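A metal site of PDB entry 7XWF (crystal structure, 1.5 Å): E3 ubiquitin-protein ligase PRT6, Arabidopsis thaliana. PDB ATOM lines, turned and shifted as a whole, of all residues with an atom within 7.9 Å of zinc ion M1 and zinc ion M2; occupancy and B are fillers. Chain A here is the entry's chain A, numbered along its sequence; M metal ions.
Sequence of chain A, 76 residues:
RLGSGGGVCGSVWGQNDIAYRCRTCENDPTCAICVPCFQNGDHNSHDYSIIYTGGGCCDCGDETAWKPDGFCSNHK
Zinc ion M2 is bound by ND1 of His 75, SG of Cys 60, SG of Cys 72 and SG of Cys 37.
Zinc ion M2 has four donor atoms within binding distance.
The backbone NH (N) of Cys 60 lies close to the side-chain sulfur (SG) of Cys 58, at 3.4 Å.
The backbone carbonyl oxygen (O) of Cys 60 sits at hydrogen-bond distance from the backbone NH (N) of Cys 9 (3.0 Å).
O of Ser 11 sits at hydrogen-bond distance from N of Cys 58 (2.9 Å).
The backbone carbonyl oxygen of Cys 58 is in hydrogen-bond range of the backbone NH of Gly 10.
SG of Cys 9 lies close to OG of Ser 11.
The backbone NH (N) of Asn 74 lies close to the side-chain sulfur (SG) of Cys 72, 3.3 Å away.
Zinc ion M1 is bound by SG of Cys 58 (2.3 Å), SG of Cys 34 (2.3 Å), SG of Cys 9 (2.3 Å) and SG of Cys 37 (2.3 Å).
Zinc ion M1 has four donor atoms within binding distance.
Of the 30 residues printed, 4 come within 4 Å of zinc ion M1.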
ATOM      1  N   GLY A   7     -16.851   9.196 -27.940  1.00  0.00           N
ATOM      2  CA  GLY A   7     -15.415   9.162 -27.775  1.00  0.00           C
ATOM      3  C   GLY A   7     -14.780  10.525 -27.567  1.00  0.00           C
ATOM      4  O   GLY A   7     -14.882  11.410 -28.419  1.00  0.00           O
ATOM      5  N   VAL A   8     -14.130  10.711 -26.415  1.00  0.00           N
ATOM      6  CA  VAL A   8     -13.266  11.855 -26.164  1.00  0.00           C
ATOM      7  C   VAL A   8     -11.860  11.448 -26.562  1.00  0.00           C
ATOM      8  O   VAL A   8     -11.456  10.304 -26.360  1.00  0.00           O
ATOM      9  CB  VAL A   8     -13.324  12.247 -24.675  1.00  0.00           C
ATOM     10  CG1 VAL A   8     -12.279  13.306 -24.364  1.00  0.00           C
ATOM     11  CG2 VAL A   8     -14.709  12.723 -24.303  1.00  0.00           C
ATOM     12  N   CYS A   9     -11.093  12.391 -27.109  1.00  0.00           N
ATOM     13  CA  CYS A   9      -9.719  12.087 -27.500  1.00  0.00           C
ATOM     14  C   CYS A   9      -8.898  11.671 -26.281  1.00  0.00           C
ATOM     15  O   CYS A   9      -8.273  10.608 -26.267  1.00  0.00           O
ATOM     16  CB  CYS A   9      -9.074  13.301 -28.176  1.00  0.00           C
ATOM     17  SG  CYS A   9      -7.323  13.088 -28.631  1.00  0.00           S
ATOM     18  N   GLY A  10      -8.831  12.541 -25.284  1.00  0.00           N
ATOM     19  CA  GLY A  10      -8.103  12.279 -24.064  1.00  0.00           C
ATOM     20  C   GLY A  10      -6.597  12.123 -24.152  1.00  0.00           C
ATOM     21  O   GLY A  10      -5.966  11.803 -23.124  1.00  0.00           O
ATOM     22  N   SER A  11      -5.992  12.348 -25.325  1.00  0.00           N
ATOM     23  CA  SER A  11      -4.550  12.202 -25.476  1.00  0.00           C
ATOM     24  C   SER A  11      -3.833  13.112 -24.494  1.00  0.00           C
ATOM     25  O   SER A  11      -4.245  14.256 -24.281  1.00  0.00           O
ATOM     26  CB  SER A  11      -4.136  12.612 -26.889  1.00  0.00           C
ATOM     27  OG  SER A  11      -4.497  11.612 -27.833  1.00  0.00           O
ATOM     28  N   VAL A  12      -2.718  12.639 -23.941  1.00  0.00           N
ATOM     29  CA  VAL A  12      -2.077  13.270 -22.794  1.00  0.00           C
ATOM     30  C   VAL A  12      -0.775  13.937 -23.187  1.00  0.00           C
ATOM     31  O   VAL A  12       0.022  13.373 -23.940  1.00  0.00           O
ATOM     32  CB  VAL A  12      -1.875  12.262 -21.644  1.00  0.00           C
ATOM     33  CG1 VAL A  12      -1.081  12.900 -20.499  1.00  0.00           C
ATOM     34  CG2 VAL A  12      -3.198  11.713 -21.172  1.00  0.00           C
ATOM     35  N   TRP A  13      -0.544  15.134 -22.646  1.00  0.00           N
ATOM     36  CA  TRP A  13       0.666  15.894 -22.901  1.00  0.00           C
ATOM     37  C   TRP A  13       1.590  15.829 -21.704  1.00  0.00           C
ATOM     38  O   TRP A  13       1.132  15.801 -20.561  1.00  0.00           O
ATOM     39  CB  TRP A  13       0.377  17.383 -23.150  1.00  0.00           C
ATOM     40  CG  TRP A  13      -0.543  17.598 -24.238  1.00  0.00           C
ATOM     41  CD1 TRP A  13      -0.379  17.215 -25.514  1.00  0.00           C
ATOM     42  CD2 TRP A  13      -1.823  18.212 -24.159  1.00  0.00           C
ATOM     43  NE1 TRP A  13      -1.465  17.549 -26.258  1.00  0.00           N
ATOM     44  CE2 TRP A  13      -2.381  18.166 -25.450  1.00  0.00           C
ATOM     45  CE3 TRP A  13      -2.560  18.815 -23.131  1.00  0.00           C
ATOM     46  CZ2 TRP A  13      -3.625  18.689 -25.756  1.00  0.00           C
ATOM     47  CZ3 TRP A  13      -3.816  19.333 -23.434  1.00  0.00           C
ATOM     48  CH2 TRP A  13      -4.327  19.276 -24.742  1.00  0.00           C
ATOM     49  N   ALA A  32      -7.840  22.936 -24.306  1.00  0.00           N
ATOM     50  CA  ALA A  32      -6.888  22.842 -25.404  1.00  0.00           C
ATOM     51  C   ALA A  32      -7.141  21.565 -26.184  1.00  0.00           C
ATOM     52  O   ALA A  32      -7.730  20.606 -25.670  1.00  0.00           O
ATOM     53  CB  ALA A  32      -5.439  22.835 -24.921  1.00  0.00           C
ATOM     54  N   ILE A  33      -6.643  21.522 -27.414  1.00  0.00           N
ATOM     55  CA  ILE A  33      -6.719  20.294 -28.185  1.00  0.00           C
ATOM     56  C   ILE A  33      -5.352  19.956 -28.771  1.00  0.00           C
ATOM     57  O   ILE A  33      -4.522  20.827 -29.032  1.00  0.00           O
ATOM     58  CB  ILE A  33      -7.800  20.274 -29.266  1.00  0.00           C
ATOM     59  CG1 ILE A  33      -7.603  21.400 -30.260  1.00  0.00           C
ATOM     60  CG2 ILE A  33      -9.177  20.338 -28.589  1.00  0.00           C
ATOM     61  CD1 ILE A  33      -8.567  21.296 -31.453  1.00  0.00           C
ATOM     62  N   CYS A  34      -5.158  18.671 -28.997  1.00  0.00           N
ATOM     63  CA  CYS A  34      -3.898  18.170 -29.516  1.00  0.00           C
ATOM     64  C   CYS A  34      -3.715  18.570 -30.979  1.00  0.00           C
ATOM     65  O   CYS A  34      -4.673  18.887 -31.700  1.00  0.00           O
ATOM     66  CB  CYS A  34      -3.803  16.662 -29.297  1.00  0.00           C
ATOM     67  SG  CYS A  34      -4.827  15.632 -30.369  1.00  0.00           S
ATOM     68  N   VAL A  35      -2.458  18.564 -31.422  1.00  0.00           N
ATOM     69  CA  VAL A  35      -2.181  18.971 -32.795  1.00  0.00           C
ATOM     70  C   VAL A  35      -2.963  18.147 -33.807  1.00  0.00           C
ATOM     71  O   VAL A  35      -3.559  18.734 -34.724  1.00  0.00           O
ATOM     72  CB  VAL A  35      -0.654  18.987 -33.038  1.00  0.00           C
ATOM     73  CG1 VAL A  35      -0.382  19.256 -34.508  1.00  0.00           C
ATOM     74  CG2 VAL A  35       0.022  20.020 -32.160  1.00  0.00           C
ATOM     75  N   PRO A  36      -2.972  16.813 -33.739  1.00  0.00           N
ATOM     76  CA  PRO A  36      -3.763  16.059 -34.736  1.00  0.00           C
ATOM     77  C   PRO A  36      -5.240  16.416 -34.749  1.00  0.00           C
ATOM     78  O   PRO A  36      -5.833  16.532 -35.833  1.00  0.00           O
ATOM     79  CB  PRO A  36      -3.536  14.593 -34.338  1.00  0.00           C
ATOM     80  CG  PRO A  36      -2.298  14.593 -33.496  1.00  0.00           C
ATOM     81  CD  PRO A  36      -2.195  15.934 -32.851  1.00  0.00           C
ATOM     82  N   CYS A  37      -5.838  16.618 -33.578  1.00  0.00           N
ATOM     83  CA  CYS A  37      -7.246  17.017 -33.519  1.00  0.00           C
ATOM     84  C   CYS A  37      -7.433  18.406 -34.122  1.00  0.00           C
ATOM     85  O   CYS A  37      -8.393  18.637 -34.868  1.00  0.00           O
ATOM     86  CB  CYS A  37      -7.761  16.961 -32.090  1.00  0.00           C
ATOM     87  SG  CYS A  37      -8.076  15.265 -31.499  1.00  0.00           S
ATOM     88  N   PHE A  38      -6.511  19.336 -33.862  1.00  0.00           N
ATOM     89  CA  PHE A  38      -6.577  20.626 -34.517  1.00  0.00           C
ATOM     90  C   PHE A  38      -6.552  20.494 -36.037  1.00  0.00           C
ATOM     91  O   PHE A  38      -7.342  21.119 -36.743  1.00  0.00           O
ATOM     92  CB  PHE A  38      -5.456  21.533 -34.034  1.00  0.00           C
ATOM     93  CG  PHE A  38      -5.517  22.907 -34.623  1.00  0.00           C
ATOM     94  CD1 PHE A  38      -6.322  23.878 -34.041  1.00  0.00           C
ATOM     95  CD2 PHE A  38      -4.795  23.242 -35.770  1.00  0.00           C
ATOM     96  CE1 PHE A  38      -6.387  25.153 -34.583  1.00  0.00           C
ATOM     97  CE2 PHE A  38      -4.873  24.512 -36.309  1.00  0.00           C
ATOM     98  CZ  PHE A  38      -5.659  25.463 -35.714  1.00  0.00           C
ATOM     99  N   ASN A  40      -7.341  18.029 -37.975  1.00  0.00           N
ATOM    100  CA  ASN A  40      -8.468  17.329 -38.568  1.00  0.00           C
ATOM    101  C   ASN A  40      -9.800  17.992 -38.254  1.00  0.00           C
ATOM    102  O   ASN A  40     -10.853  17.373 -38.433  1.00  0.00           O
ATOM    103  CB  ASN A  40      -8.449  15.880 -38.127  1.00  0.00           C
ATOM    104  CG  ASN A  40      -7.298  15.114 -38.744  1.00  0.00           C
ATOM    105  OD1 ASN A  40      -7.022  15.239 -39.934  1.00  0.00           O
ATOM    106  ND2 ASN A  40      -6.633  14.322 -37.924  1.00  0.00           N
ATOM    107  N   GLY A  41      -9.779  19.257 -37.830  1.00  0.00           N
ATOM    108  CA  GLY A  41     -10.986  20.033 -37.659  1.00  0.00           C
ATOM    109  C   GLY A  41     -10.896  21.323 -38.456  1.00  0.00           C
ATOM    110  O   GLY A  41      -9.939  21.545 -39.205  1.00  0.00           O
ATOM    111  N   CYS A  57      -4.637  17.108 -20.970  1.00  0.00           N
ATOM    112  CA  CYS A  57      -5.230  16.172 -21.898  1.00  0.00           C
ATOM    113  C   CYS A  57      -6.118  16.897 -22.896  1.00  0.00           C
ATOM    114  O   CYS A  57      -6.695  17.949 -22.609  1.00  0.00           O
ATOM    115  CB  CYS A  57      -5.983  15.018 -21.212  1.00  0.00           C
ATOM    116  SG  CYS A  57      -7.424  15.420 -20.214  1.00  0.00           S
ATOM    117  N   CYS A  58      -6.251  16.285 -24.072  1.00  0.00           N
ATOM    118  CA  CYS A  58      -6.992  16.901 -25.164  1.00  0.00           C
ATOM    119  C   CYS A  58      -8.496  16.873 -24.877  1.00  0.00           C
ATOM    120  O   CYS A  58      -9.071  15.857 -24.472  1.00  0.00           O
ATOM    121  CB  CYS A  58      -6.746  16.161 -26.473  1.00  0.00           C
ATOM    122  SG  CYS A  58      -7.578  16.712 -27.919  1.00  0.00           S
ATOM    123  N   ASP A  59      -9.134  17.987 -25.205  1.00  0.00           N
ATOM    124  CA  ASP A  59     -10.554  18.185 -24.935  1.00  0.00           C
ATOM    125  C   ASP A  59     -11.445  17.893 -26.139  1.00  0.00           C
ATOM    126  O   ASP A  59     -12.667  17.994 -26.028  1.00  0.00           O
ATOM    127  CB  ASP A  59     -10.770  19.638 -24.504  1.00  0.00           C
ATOM    128  CG  ASP A  59     -10.173  19.939 -23.138  1.00  0.00           C
ATOM    129  OD1 ASP A  59     -10.394  19.125 -22.210  1.00  0.00           O
ATOM    130  OD2 ASP A  59      -9.515  20.985 -22.980  1.00  0.00           O
ATOM    131  N   CYS A  60     -10.839  17.521 -27.268  1.00  0.00           N
ATOM    132  CA  CYS A  60     -11.601  17.268 -28.483  1.00  0.00           C
ATOM    133  C   CYS A  60     -12.582  16.116 -28.258  1.00  0.00           C
ATOM    134  O   CYS A  60     -12.203  15.051 -27.782  1.00  0.00           O
ATOM    135  CB  CYS A  60     -10.662  16.929 -29.630  1.00  0.00           C
ATOM    136  SG  CYS A  60     -11.522  16.746 -31.195  1.00  0.00           S
ATOM    137  N   GLY A  61     -13.862  16.359 -28.570  1.00  0.00           N
ATOM    138  CA  GLY A  61     -14.899  15.377 -28.362  1.00  0.00           C
ATOM    139  C   GLY A  61     -15.653  15.514 -27.062  1.00  0.00           C
ATOM    140  O   GLY A  61     -16.701  14.870 -26.887  1.00  0.00           O
ATOM    141  N   ASP A  62     -15.167  16.347 -26.141  1.00  0.00           N
ATOM    142  CA  ASP A  62     -15.815  16.590 -24.843  1.00  0.00           C
ATOM    143  C   ASP A  62     -16.551  17.917 -24.915  1.00  0.00           C
ATOM    144  O   ASP A  62     -15.958  18.982 -24.768  1.00  0.00           O
ATOM    145  CB  ASP A  62     -14.747  16.627 -23.755  1.00  0.00           C
ATOM    146  CG  ASP A  62     -15.311  16.883 -22.373  1.00  0.00           C
ATOM    147  OD1 ASP A  62     -16.552  17.025 -22.238  1.00  0.00           O
ATOM    148  OD2 ASP A  62     -14.523  16.933 -21.401  1.00  0.00           O
ATOM    149  N   TRP A  66     -15.192  21.830 -24.890  1.00  0.00           N
ATOM    150  CA  TRP A  66     -14.906  22.287 -26.236  1.00  0.00           C
ATOM    151  C   TRP A  66     -16.200  22.333 -27.033  1.00  0.00           C
ATOM    152  O   TRP A  66     -17.031  21.414 -26.938  1.00  0.00           O
ATOM    153  CB  TRP A  66     -13.899  21.346 -26.873  1.00  0.00           C
ATOM    154  CG  TRP A  66     -13.117  21.863 -28.016  1.00  0.00           C
ATOM    155  CD1 TRP A  66     -13.327  21.612 -29.340  1.00  0.00           C
ATOM    156  CD2 TRP A  66     -11.919  22.660 -27.944  1.00  0.00           C
ATOM    157  NE1 TRP A  66     -12.365  22.241 -30.104  1.00  0.00           N
ATOM    158  CE2 TRP A  66     -11.492  22.896 -29.264  1.00  0.00           C
ATOM    159  CE3 TRP A  66     -11.193  23.222 -26.887  1.00  0.00           C
ATOM    160  CZ2 TRP A  66     -10.343  23.630 -29.558  1.00  0.00           C
ATOM    161  CZ3 TRP A  66     -10.080  23.984 -27.187  1.00  0.00           C
ATOM    162  CH2 TRP A  66      -9.669  24.183 -28.509  1.00  0.00           C
ATOM    163  N   GLY A  70     -16.021  22.682 -33.098  1.00  0.00           N
ATOM    164  CA  GLY A  70     -14.575  22.582 -33.074  1.00  0.00           C
ATOM    165  C   GLY A  70     -14.020  21.193 -32.916  1.00  0.00           C
ATOM    166  O   GLY A  70     -12.786  21.056 -32.794  1.00  0.00           O
ATOM    167  N   PHE A  71     -14.862  20.162 -32.933  1.00  0.00           N
ATOM    168  CA  PHE A  71     -14.384  18.790 -32.877  1.00  0.00           C
ATOM    169  C   PHE A  71     -13.781  18.404 -34.218  1.00  0.00           C
ATOM    170  O   PHE A  71     -14.170  18.900 -35.276  1.00  0.00           O
ATOM    171  CB  PHE A  71     -15.562  17.828 -32.635  1.00  0.00           C
ATOM    172  CG  PHE A  71     -16.174  17.908 -31.259  1.00  0.00           C
ATOM    173  CD1 PHE A  71     -17.306  17.166 -30.971  1.00  0.00           C
ATOM    174  CD2 PHE A  71     -15.635  18.713 -30.253  1.00  0.00           C
ATOM    175  CE1 PHE A  71     -17.901  17.209 -29.723  1.00  0.00           C
ATOM    176  CE2 PHE A  71     -16.218  18.751 -28.998  1.00  0.00           C
ATOM    177  CZ  PHE A  71     -17.348  17.997 -28.724  1.00  0.00           C
ATOM    178  N   CYS A  72     -12.812  17.511 -34.171  1.00  0.00           N
ATOM    179  CA  CYS A  72     -12.238  16.957 -35.385  1.00  0.00           C
ATOM    180  C   CYS A  72     -13.103  15.823 -35.930  1.00  0.00           C
ATOM    181  O   CYS A  72     -14.053  15.370 -35.286  1.00  0.00           O
ATOM    182  CB  CYS A  72     -10.806  16.458 -35.130  1.00  0.00           C
ATOM    183  SG  CYS A  72     -10.681  14.805 -34.375  1.00  0.00           S
ATOM    184  N   SER A  73     -12.723  15.348 -37.105  1.00  0.00           N
ATOM    185  CA  SER A  73     -13.511  14.327 -37.801  1.00  0.00           C
ATOM    186  C   SER A  73     -13.528  12.985 -37.088  1.00  0.00           C
ATOM    187  O   SER A  73     -14.406  12.157 -37.386  1.00  0.00           O
ATOM    188  CB  SER A  73     -12.990  14.126 -39.213  1.00  0.00           C
ATOM    189  OG  SER A  73     -11.609  13.782 -39.223  1.00  0.00           O
ATOM    190  N   ASN A  74     -12.623  12.739 -36.159  1.00  0.00           N
ATOM    191  CA  ASN A  74     -12.576  11.446 -35.488  1.00  0.00           C
ATOM    192  C   ASN A  74     -13.291  11.432 -34.151  1.00  0.00           C
ATOM    193  O   ASN A  74     -13.451  10.348 -33.574  1.00  0.00           O
ATOM    194  CB  ASN A  74     -11.113  11.012 -35.294  1.00  0.00           C
ATOM    195  CG  ASN A  74     -10.393  10.836 -36.603  1.00  0.00           C
ATOM    196  OD1 ASN A  74     -10.905  10.215 -37.542  1.00  0.00           O
ATOM    197  ND2 ASN A  74      -9.194  11.374 -36.681  1.00  0.00           N
ATOM    198  N   HIS A  75     -13.772  12.575 -33.655  1.00  0.00           N
ATOM    199  CA  HIS A  75     -14.354  12.653 -32.319  1.00  0.00           C
ATOM    200  C   HIS A  75     -15.733  13.273 -32.326  1.00  0.00           C
ATOM    201  O   HIS A  75     -16.118  13.980 -31.384  1.00  0.00           O
ATOM    202  CB  HIS A  75     -13.415  13.373 -31.350  1.00  0.00           C
ATOM    203  CG  HIS A  75     -12.124  12.644 -31.168  1.00  0.00           C
ATOM    204  ND1 HIS A  75     -10.922  13.170 -31.566  1.00  0.00           N
ATOM    205  CD2 HIS A  75     -11.865  11.404 -30.708  1.00  0.00           C
ATOM    206  CE1 HIS A  75      -9.961  12.296 -31.344  1.00  0.00           C
ATOM    207  NE2 HIS A  75     -10.510  11.207 -30.811  1.00  0.00           N
ATOM    208  N   LYS A  76     -16.514  13.012 -33.368  1.00  0.00           N
ATOM    209  CA  LYS A  76     -17.900  13.445 -33.320  1.00  0.00           C
ATOM    210  C   LYS A  76     -18.892  12.304 -33.544  1.00  0.00           C
ATOM    211  O   LYS A  76     -20.076  12.446 -33.226  1.00  0.00           O
ATOM    212  CB  LYS A  76     -18.220  14.589 -34.265  1.00  0.00           C
ATOM    213  CG  LYS A  76     -17.282  14.878 -35.398  1.00  0.00           C
ATOM    214  CD  LYS A  76     -17.688  16.194 -36.034  1.00  0.00           C
ATOM    215  CE  LYS A  76     -16.714  16.672 -37.050  1.00  0.00           C
ATOM    216  NZ  LYS A  76     -17.119  17.922 -37.697  1.00  0.00           N
HETATM  217 ZN    ZN M   1      -6.902  15.196 -29.467  1.00  0.00          ZN
HETATM  218 ZN    ZN M   2     -10.387  15.048 -32.095  1.00  0.00          ZN
